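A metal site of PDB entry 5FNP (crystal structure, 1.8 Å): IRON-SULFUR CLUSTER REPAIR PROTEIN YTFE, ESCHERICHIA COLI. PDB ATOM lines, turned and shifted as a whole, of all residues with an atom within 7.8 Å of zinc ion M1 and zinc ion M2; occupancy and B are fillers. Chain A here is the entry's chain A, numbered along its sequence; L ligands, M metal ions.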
ATOM      1  N   ILE A  79      -8.754  10.600  23.111  1.00  0.00           N
ATOM      2  CA  ILE A  79      -8.651   9.625  24.209  1.00  0.00           C
ATOM      3  C   ILE A  79      -7.195   9.316  24.538  1.00  0.00           C
ATOM      4  O   ILE A  79      -6.797   9.307  25.716  1.00  0.00           O
ATOM      5  CB  ILE A  79      -9.420   8.360  23.883  1.00  0.00           C
ATOM      6  CG1 ILE A  79     -10.929   8.662  23.937  1.00  0.00           C
ATOM      7  CG2 ILE A  79      -9.104   7.259  24.880  1.00  0.00           C
ATOM      8  CD1 ILE A  79     -11.766   7.564  23.320  1.00  0.00           C
ATOM      9  N   ILE A  80      -6.422   8.995  23.518  1.00  0.00           N
ATOM     10  CA  ILE A  80      -5.035   8.567  23.732  1.00  0.00           C
ATOM     11  C   ILE A  80      -4.272   9.644  24.490  1.00  0.00           C
ATOM     12  O   ILE A  80      -3.552   9.345  25.477  1.00  0.00           O
ATOM     13  CB  ILE A  80      -4.325   8.203  22.406  1.00  0.00           C
ATOM     14  CG1 ILE A  80      -4.902   6.912  21.834  1.00  0.00           C
ATOM     15  CG2 ILE A  80      -2.815   8.041  22.608  1.00  0.00           C
ATOM     16  CD1 ILE A  80      -4.608   6.701  20.364  1.00  0.00           C
ATOM     17  N   TYR A  83      -6.540  11.230  27.901  1.00  0.00           N
ATOM     18  CA  TYR A  83      -6.802  10.269  28.946  1.00  0.00           C
ATOM     19  C   TYR A  83      -5.712   9.190  29.122  1.00  0.00           C
ATOM     20  O   TYR A  83      -5.132   9.104  30.199  1.00  0.00           O
ATOM     21  CB  TYR A  83      -8.215   9.667  28.780  1.00  0.00           C
ATOM     22  CG  TYR A  83      -9.294  10.718  28.887  1.00  0.00           C
ATOM     23  CD1 TYR A  83      -9.462  11.466  30.057  1.00  0.00           C
ATOM     24  CD2 TYR A  83     -10.158  10.957  27.836  1.00  0.00           C
ATOM     25  CE1 TYR A  83     -10.429  12.469  30.141  1.00  0.00           C
ATOM     26  CE2 TYR A  83     -11.168  11.913  27.921  1.00  0.00           C
ATOM     27  CZ  TYR A  83     -11.292  12.660  29.080  1.00  0.00           C
ATOM     28  OH  TYR A  83     -12.303  13.592  29.160  1.00  0.00           O
ATOM     29  N   HIS A  84      -5.429   8.377  28.095  1.00  0.00           N
ATOM     30  CA  HIS A  84      -4.502   7.257  28.296  1.00  0.00           C
ATOM     31  C   HIS A  84      -3.129   7.749  28.776  1.00  0.00           C
ATOM     32  O   HIS A  84      -2.620   7.282  29.777  1.00  0.00           O
ATOM     33  CB  HIS A  84      -4.296   6.458  27.033  1.00  0.00           C
ATOM     34  CG  HIS A  84      -5.491   5.668  26.615  1.00  0.00           C
ATOM     35  ND1 HIS A  84      -5.407   4.674  25.667  1.00  0.00           N
ATOM     36  CD2 HIS A  84      -6.761   5.639  27.084  1.00  0.00           C
ATOM     37  CE1 HIS A  84      -6.589   4.077  25.553  1.00  0.00           C
ATOM     38  NE2 HIS A  84      -7.420   4.632  26.399  1.00  0.00           N
ATOM     39  N   HIS A  87      -3.298   9.083  32.378  1.00  0.00           N
ATOM     40  CA  HIS A  87      -3.376   8.014  33.390  1.00  0.00           C
ATOM     41  C   HIS A  87      -1.989   7.396  33.617  1.00  0.00           C
ATOM     42  O   HIS A  87      -1.636   7.089  34.741  1.00  0.00           O
ATOM     43  CB  HIS A  87      -4.356   6.904  33.006  1.00  0.00           C
ATOM     44  CG  HIS A  87      -5.779   7.352  32.799  1.00  0.00           C
ATOM     45  ND1 HIS A  87      -6.348   8.401  33.484  1.00  0.00           N
ATOM     46  CD2 HIS A  87      -6.769   6.835  32.035  1.00  0.00           C
ATOM     47  CE1 HIS A  87      -7.605   8.540  33.125  1.00  0.00           C
ATOM     48  NE2 HIS A  87      -7.888   7.622  32.234  1.00  0.00           N
ATOM     49  N   LEU A 126      -5.239  -1.233  34.005  1.00  0.00           N
ATOM     50  CA  LEU A 126      -5.511  -0.196  33.063  1.00  0.00           C
ATOM     51  C   LEU A 126      -4.426  -0.110  31.992  1.00  0.00           C
ATOM     52  O   LEU A 126      -4.712   0.095  30.817  1.00  0.00           O
ATOM     53  CB  LEU A 126      -5.701   1.129  33.765  1.00  0.00           C
ATOM     54  CG  LEU A 126      -6.325   2.303  33.071  1.00  0.00           C
ATOM     55  CD1 LEU A 126      -7.757   1.982  32.668  1.00  0.00           C
ATOM     56  CD2 LEU A 126      -6.278   3.485  34.024  1.00  0.00           C
ATOM     57  N   HIS A 129      -4.998  -2.937  29.478  1.00  0.00           N
ATOM     58  CA  HIS A 129      -6.228  -2.579  28.762  1.00  0.00           C
ATOM     59  C   HIS A 129      -6.005  -1.488  27.709  1.00  0.00           C
ATOM     60  O   HIS A 129      -6.413  -1.639  26.556  1.00  0.00           O
ATOM     61  CB  HIS A 129      -7.326  -2.170  29.793  1.00  0.00           C
ATOM     62  CG  HIS A 129      -8.560  -1.561  29.215  1.00  0.00           C
ATOM     63  ND1 HIS A 129      -9.733  -2.291  29.039  1.00  0.00           N
ATOM     64  CD2 HIS A 129      -8.864  -0.282  28.886  1.00  0.00           C
ATOM     65  CE1 HIS A 129     -10.676  -1.484  28.591  1.00  0.00           C
ATOM     66  NE2 HIS A 129     -10.182  -0.260  28.484  1.00  0.00           N
ATOM     67  N   MET A 130      -5.369  -0.381  28.105  1.00  0.00           N
ATOM     68  CA  MET A 130      -5.104   0.729  27.211  1.00  0.00           C
ATOM     69  C   MET A 130      -4.204   0.322  26.032  1.00  0.00           C
ATOM     70  O   MET A 130      -4.382   0.798  24.925  1.00  0.00           O
ATOM     71  CB  MET A 130      -4.501   1.909  27.940  1.00  0.00           C
ATOM     72  CG  MET A 130      -5.508   2.530  28.901  1.00  0.00           C
ATOM     73  SD  MET A 130      -4.984   4.035  29.734  1.00  0.00           S
ATOM     74  CE  MET A 130      -3.503   3.447  30.556  1.00  0.00           C
ATOM     75  N   MET A 131      -3.232  -0.544  26.297  1.00  0.00           N
ATOM     76  CA  MET A 131      -2.339  -1.045  25.231  1.00  0.00           C
ATOM     77  C   MET A 131      -3.109  -1.845  24.196  1.00  0.00           C
ATOM     78  O   MET A 131      -2.879  -1.719  23.011  1.00  0.00           O
ATOM     79  CB  MET A 131      -1.198  -1.907  25.797  1.00  0.00           C
ATOM     80  CG  MET A 131      -0.180  -2.394  24.755  1.00  0.00           C
ATOM     81  SD  MET A 131       1.079  -3.454  25.485  1.00  0.00           S
ATOM     82  CE  MET A 131       0.270  -5.041  25.346  1.00  0.00           C
ATOM     83  N   GLU A 133      -6.293  -1.446  23.453  1.00  0.00           N
ATOM     84  CA  GLU A 133      -7.023  -0.464  22.692  1.00  0.00           C
ATOM     85  C   GLU A 133      -6.150   0.217  21.648  1.00  0.00           C
ATOM     86  O   GLU A 133      -6.539   0.418  20.488  1.00  0.00           O
ATOM     87  CB  GLU A 133      -7.673   0.585  23.595  1.00  0.00           C
ATOM     88  CG  GLU A 133      -8.848   0.026  24.406  1.00  0.00           C
ATOM     89  CD  GLU A 133      -9.508   1.017  25.375  1.00  0.00           C
ATOM     90  OE1 GLU A 133      -8.893   2.086  25.667  1.00  0.00           O
ATOM     91  OE2 GLU A 133     -10.652   0.742  25.874  1.00  0.00           O
ATOM     92  N   GLU A 134      -4.961   0.614  22.073  1.00  0.00           N
ATOM     93  CA  GLU A 134      -4.071   1.352  21.160  1.00  0.00           C
ATOM     94  C   GLU A 134      -3.504   0.495  20.042  1.00  0.00           C
ATOM     95  O   GLU A 134      -3.276   1.015  18.933  1.00  0.00           O
ATOM     96  CB  GLU A 134      -2.950   2.064  21.957  1.00  0.00           C
ATOM     97  CG  GLU A 134      -3.510   3.266  22.731  1.00  0.00           C
ATOM     98  CD  GLU A 134      -2.496   3.954  23.640  1.00  0.00           C
ATOM     99  OE1 GLU A 134      -1.308   4.033  23.265  1.00  0.00           O
ATOM    100  OE2 GLU A 134      -2.867   4.420  24.747  1.00  0.00           O
ATOM    101  N   LEU A 137      -7.888  -2.235  18.853  1.00  0.00           N
ATOM    102  CA  LEU A 137      -9.235  -1.691  18.673  1.00  0.00           C
ATOM    103  C   LEU A 137      -9.262  -0.341  18.011  1.00  0.00           C
ATOM    104  O   LEU A 137     -10.007  -0.117  17.042  1.00  0.00           O
ATOM    105  CB  LEU A 137      -9.983  -1.628  19.996  1.00  0.00           C
ATOM    106  CG  LEU A 137     -11.400  -1.054  19.904  1.00  0.00           C
ATOM    107  CD1 LEU A 137     -12.243  -1.882  18.939  1.00  0.00           C
ATOM    108  CD2 LEU A 137     -11.987  -1.085  21.294  1.00  0.00           C
ATOM    109  N   PHE A 138      -8.432   0.574  18.465  1.00  0.00           N
ATOM    110  CA  PHE A 138      -8.406   1.905  17.877  1.00  0.00           C
ATOM    111  C   PHE A 138      -7.921   1.893  16.387  1.00  0.00           C
ATOM    112  O   PHE A 138      -8.597   2.472  15.520  1.00  0.00           O
ATOM    113  CB  PHE A 138      -7.592   2.872  18.750  1.00  0.00           C
ATOM    114  CG  PHE A 138      -8.219   3.202  20.102  1.00  0.00           C
ATOM    115  CD1 PHE A 138      -9.526   2.793  20.473  1.00  0.00           C
ATOM    116  CD2 PHE A 138      -7.530   3.999  21.008  1.00  0.00           C
ATOM    117  CE1 PHE A 138     -10.051   3.134  21.696  1.00  0.00           C
ATOM    118  CE2 PHE A 138      -8.088   4.387  22.221  1.00  0.00           C
ATOM    119  CZ  PHE A 138      -9.340   3.926  22.581  1.00  0.00           C
ATOM    120  N   MET A 156     -13.576  -5.045  26.279  1.00  0.00           N
ATOM    121  CA  MET A 156     -13.198  -3.732  26.832  1.00  0.00           C
ATOM    122  C   MET A 156     -14.292  -3.211  27.766  1.00  0.00           C
ATOM    123  O   MET A 156     -14.000  -2.657  28.811  1.00  0.00           O
ATOM    124  CB  MET A 156     -12.890  -2.704  25.729  1.00  0.00           C
ATOM    125  CG  MET A 156     -11.654  -3.006  24.854  1.00  0.00           C
ATOM    126  SD  MET A 156     -10.097  -3.274  25.744  1.00  0.00           S
ATOM    127  CE  MET A 156     -10.049  -5.038  26.047  1.00  0.00           C
ATOM    128  N   GLU A 157     -15.586  -3.415  27.414  1.00  0.00           N
ATOM    129  CA  GLU A 157     -16.662  -2.979  28.316  1.00  0.00           C
ATOM    130  C   GLU A 157     -16.708  -3.739  29.637  1.00  0.00           C
ATOM    131  O   GLU A 157     -16.927  -3.167  30.685  1.00  0.00           O
ATOM    132  CB  GLU A 157     -18.022  -2.995  27.626  1.00  0.00           C
ATOM    133  CG  GLU A 157     -18.073  -1.903  26.552  1.00  0.00           C
ATOM    134  CD  GLU A 157     -19.452  -1.684  25.953  1.00  0.00           C
ATOM    135  OE1 GLU A 157     -20.335  -2.519  26.150  1.00  0.00           O
ATOM    136  OE2 GLU A 157     -19.643  -0.671  25.260  1.00  0.00           O
ATOM    137  N   GLU A 159     -14.073  -4.990  31.031  1.00  0.00           N
ATOM    138  CA  GLU A 159     -12.937  -4.444  31.783  1.00  0.00           C
ATOM    139  C   GLU A 159     -13.214  -3.046  32.329  1.00  0.00           C
ATOM    140  O   GLU A 159     -12.772  -2.709  33.428  1.00  0.00           O
ATOM    141  CB  GLU A 159     -11.643  -4.474  30.926  1.00  0.00           C
ATOM    142  CG  GLU A 159     -11.178  -5.918  30.703  1.00  0.00           C
ATOM    143  CD  GLU A 159      -9.961  -6.072  29.794  1.00  0.00           C
ATOM    144  OE1 GLU A 159      -9.461  -5.099  29.220  1.00  0.00           O
ATOM    145  OE2 GLU A 159      -9.572  -7.225  29.590  1.00  0.00           O
ATOM    146  N   HIS A 160     -13.978  -2.249  31.631  1.00  0.00           N
ATOM    147  CA  HIS A 160     -14.408  -0.987  32.203  1.00  0.00           C
ATOM    148  C   HIS A 160     -15.206  -1.185  33.474  1.00  0.00           C
ATOM    149  O   HIS A 160     -15.039  -0.410  34.432  1.00  0.00           O
ATOM    150  CB  HIS A 160     -15.268  -0.174  31.238  1.00  0.00           C
ATOM    151  CG  HIS A 160     -14.500   0.330  30.053  1.00  0.00           C
ATOM    152  ND1 HIS A 160     -15.121   0.823  28.937  1.00  0.00           N
ATOM    153  CD2 HIS A 160     -13.172   0.400  29.819  1.00  0.00           C
ATOM    154  CE1 HIS A 160     -14.200   1.202  28.052  1.00  0.00           C
ATOM    155  NE2 HIS A 160     -13.020   0.920  28.559  1.00  0.00           N
ATOM    156  N   LEU A 201     -11.046   9.256  34.504  1.00  0.00           N
ATOM    157  CA  LEU A 201     -11.362   7.865  34.130  1.00  0.00           C
ATOM    158  C   LEU A 201     -12.856   7.685  33.810  1.00  0.00           C
ATOM    159  O   LEU A 201     -13.233   7.007  32.837  1.00  0.00           O
ATOM    160  CB  LEU A 201     -10.844   6.906  35.221  1.00  0.00           C
ATOM    161  CG  LEU A 201     -10.734   5.421  34.926  1.00  0.00           C
ATOM    162  CD1 LEU A 201     -10.165   5.086  33.577  1.00  0.00           C
ATOM    163  CD2 LEU A 201      -9.937   4.738  36.068  1.00  0.00           C
ATOM    164  N   HIS A 204     -13.390   9.408  30.394  1.00  0.00           N
ATOM    165  CA  HIS A 204     -12.746   8.524  29.413  1.00  0.00           C
ATOM    166  C   HIS A 204     -13.654   7.319  29.109  1.00  0.00           C
ATOM    167  O   HIS A 204     -13.951   7.024  27.955  1.00  0.00           O
ATOM    168  CB  HIS A 204     -11.406   8.103  30.038  1.00  0.00           C
ATOM    169  CG  HIS A 204     -10.655   6.972  29.375  1.00  0.00           C
ATOM    170  ND1 HIS A 204      -9.623   6.368  30.040  1.00  0.00           N
ATOM    171  CD2 HIS A 204     -10.754   6.337  28.188  1.00  0.00           C
ATOM    172  CE1 HIS A 204      -9.103   5.421  29.303  1.00  0.00           C
ATOM    173  NE2 HIS A 204      -9.759   5.378  28.155  1.00  0.00           N
ATOM    174  N   ILE A 205     -14.069   6.628  30.171  1.00  0.00           N
ATOM    175  CA  ILE A 205     -14.933   5.439  29.974  1.00  0.00           C
ATOM    176  C   ILE A 205     -16.259   5.841  29.344  1.00  0.00           C
ATOM    177  O   ILE A 205     -16.747   5.106  28.479  1.00  0.00           O
ATOM    178  CB  ILE A 205     -15.096   4.633  31.248  1.00  0.00           C
ATOM    179  CG1 ILE A 205     -13.744   3.927  31.557  1.00  0.00           C
ATOM    180  CG2 ILE A 205     -16.202   3.551  31.108  1.00  0.00           C
ATOM    181  CD1 ILE A 205     -13.671   3.385  32.938  1.00  0.00           C
ATOM    182  N   GLU A 208     -15.792   6.290  25.638  1.00  0.00           N
ATOM    183  CA  GLU A 208     -15.700   4.995  24.962  1.00  0.00           C
ATOM    184  C   GLU A 208     -17.061   4.262  24.916  1.00  0.00           C
ATOM    185  O   GLU A 208     -17.560   3.901  23.844  1.00  0.00           O
ATOM    186  CB  GLU A 208     -14.632   4.132  25.613  1.00  0.00           C
ATOM    187  CG  GLU A 208     -13.247   4.665  25.252  1.00  0.00           C
ATOM    188  CD  GLU A 208     -12.066   3.979  25.921  1.00  0.00           C
ATOM    189  OE1 GLU A 208     -12.231   3.018  26.686  1.00  0.00           O
ATOM    190  OE2 GLU A 208     -10.912   4.460  25.682  1.00  0.00           O
ATOM    191  N   ASN A 209     -17.639   4.047  26.081  1.00  0.00           N
ATOM    192  CA  ASN A 209     -18.877   3.265  26.174  1.00  0.00           C
ATOM    193  C   ASN A 209     -20.081   3.949  25.497  1.00  0.00           C
ATOM    194  O   ASN A 209     -20.908   3.257  24.890  1.00  0.00           O
ATOM    195  CB  ASN A 209     -19.278   3.048  27.631  1.00  0.00           C
ATOM    196  CG  ASN A 209     -18.516   1.906  28.304  1.00  0.00           C
ATOM    197  OD1 ASN A 209     -17.530   1.437  27.843  1.00  0.00           O
ATOM    198  ND2 ASN A 209     -19.064   1.434  29.403  1.00  0.00           N
ATOM    199  N   LEU A 212     -17.812   6.278  21.349  1.00  0.00           N
ATOM    200  CA  LEU A 212     -16.938   5.587  20.399  1.00  0.00           C
ATOM    201  C   LEU A 212     -17.392   4.185  20.032  1.00  0.00           C
ATOM    202  O   LEU A 212     -17.480   3.857  18.827  1.00  0.00           O
ATOM    203  CB  LEU A 212     -15.499   5.554  20.902  1.00  0.00           C
ATOM    204  CG  LEU A 212     -14.469   4.895  19.970  1.00  0.00           C
ATOM    205  CD1 LEU A 212     -14.328   5.648  18.668  1.00  0.00           C
ATOM    206  CD2 LEU A 212     -13.115   4.780  20.669  1.00  0.00           C
ATOM    207  N   PHE A 213     -17.641   3.366  21.034  1.00  0.00           N
ATOM    208  CA  PHE A 213     -17.965   1.960  20.818  1.00  0.00           C
ATOM    209  C   PHE A 213     -19.279   1.768  20.054  1.00  0.00           C
ATOM    210  O   PHE A 213     -19.266   1.065  19.042  1.00  0.00           O
ATOM    211  CB  PHE A 213     -17.956   1.173  22.133  1.00  0.00           C
ATOM    212  CG  PHE A 213     -16.576   1.062  22.810  1.00  0.00           C
ATOM    213  CD1 PHE A 213     -15.400   1.486  22.193  1.00  0.00           C
ATOM    214  CD2 PHE A 213     -16.489   0.460  24.060  1.00  0.00           C
ATOM    215  CE1 PHE A 213     -14.177   1.342  22.841  1.00  0.00           C
ATOM    216  CE2 PHE A 213     -15.253   0.297  24.702  1.00  0.00           C
ATOM    217  CZ  PHE A 213     -14.099   0.744  24.091  1.00  0.00           C
HETATM  218  O1  LIG L   1      -9.721   2.637  28.340  1.00  0.00           O
HETATM  219 ZN    ZN M   1     -11.117   1.368  27.646  1.00  0.00          ZN
HETATM  220 ZN    ZN M   2      -9.384   3.853  26.804  1.00  0.00          ZN
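A ring nitrogen (ND1) of His 84 is in hydrogen-bond range of the side-chain carboxylate (OE2) of Glu 134 (2.7 Å). The side-chain carboxylate of Glu 159 lies within hydrogen-bond range of a ring nitrogen (ND1) of His 129 (2.8 Å). The backbone carbonyl oxygen of Glu 208 lies within hydrogen-bond range of the backbone NH of Phe 213 (2.9 Å). The backbone NH (N) of His 84 is in hydrogen-bond range of the backbone carbonyl oxygen (O) of Ile 79, at 2.9 Å. A ring nitrogen (NE2) of His 87 is in hydrogen-bond range of a ring nitrogen (ND1) of His 204, 3.1 Å away. N of Phe 138 is in hydrogen-bond range of O of Glu 133 (2.8 Å). A ring nitrogen (ND1) of His 129 lies close to the side-chain sulfur (SD) of Met 156, at 3.5 Å. A ring nitrogen (ND1) of His 160 lies within hydrogen-bond range of the side-chain amide oxygen (OD1) of Asn 209.
Within 4 Å of zinc ion M1: His 129, Glu 133, His 160 and Glu 208. The nearest printed residue that does not touch zinc ion M1 is His 204 (4.3 Å).
Merely in contact with zinc ion M2: Ile 79 (3.9 Å). Of the 24 residues printed, 5 come within 4 Å of zinc ion M2. Along chain A the residues within 4 Å of zinc ion M2 span positions 79 to 208.
The side-chain carboxylate (OE2) of Glu 133 is bound to zinc ion M1 (1.9 Å). O1 of the ligand is bound to zinc ion M1, 2.0 Å away. Zinc ion M1 is bound by NE2 of His 129 (2.1 Å). NE2 of His 160 is bound to zinc ion M1, 2.2 Å away. Zinc ion M1 is bound by the side-chain carboxylate (OE1) of Glu 208 (2.2 Å). Zinc ion M1 has five donor atoms within binding distance.
Zinc ion M2 is bound by O1 of the ligand, OE2 of Glu 208, NE2 of His 204, NE2 of His 84 and OE1 of Glu 133. Zinc ion M2 has five donor atoms within binding distance.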
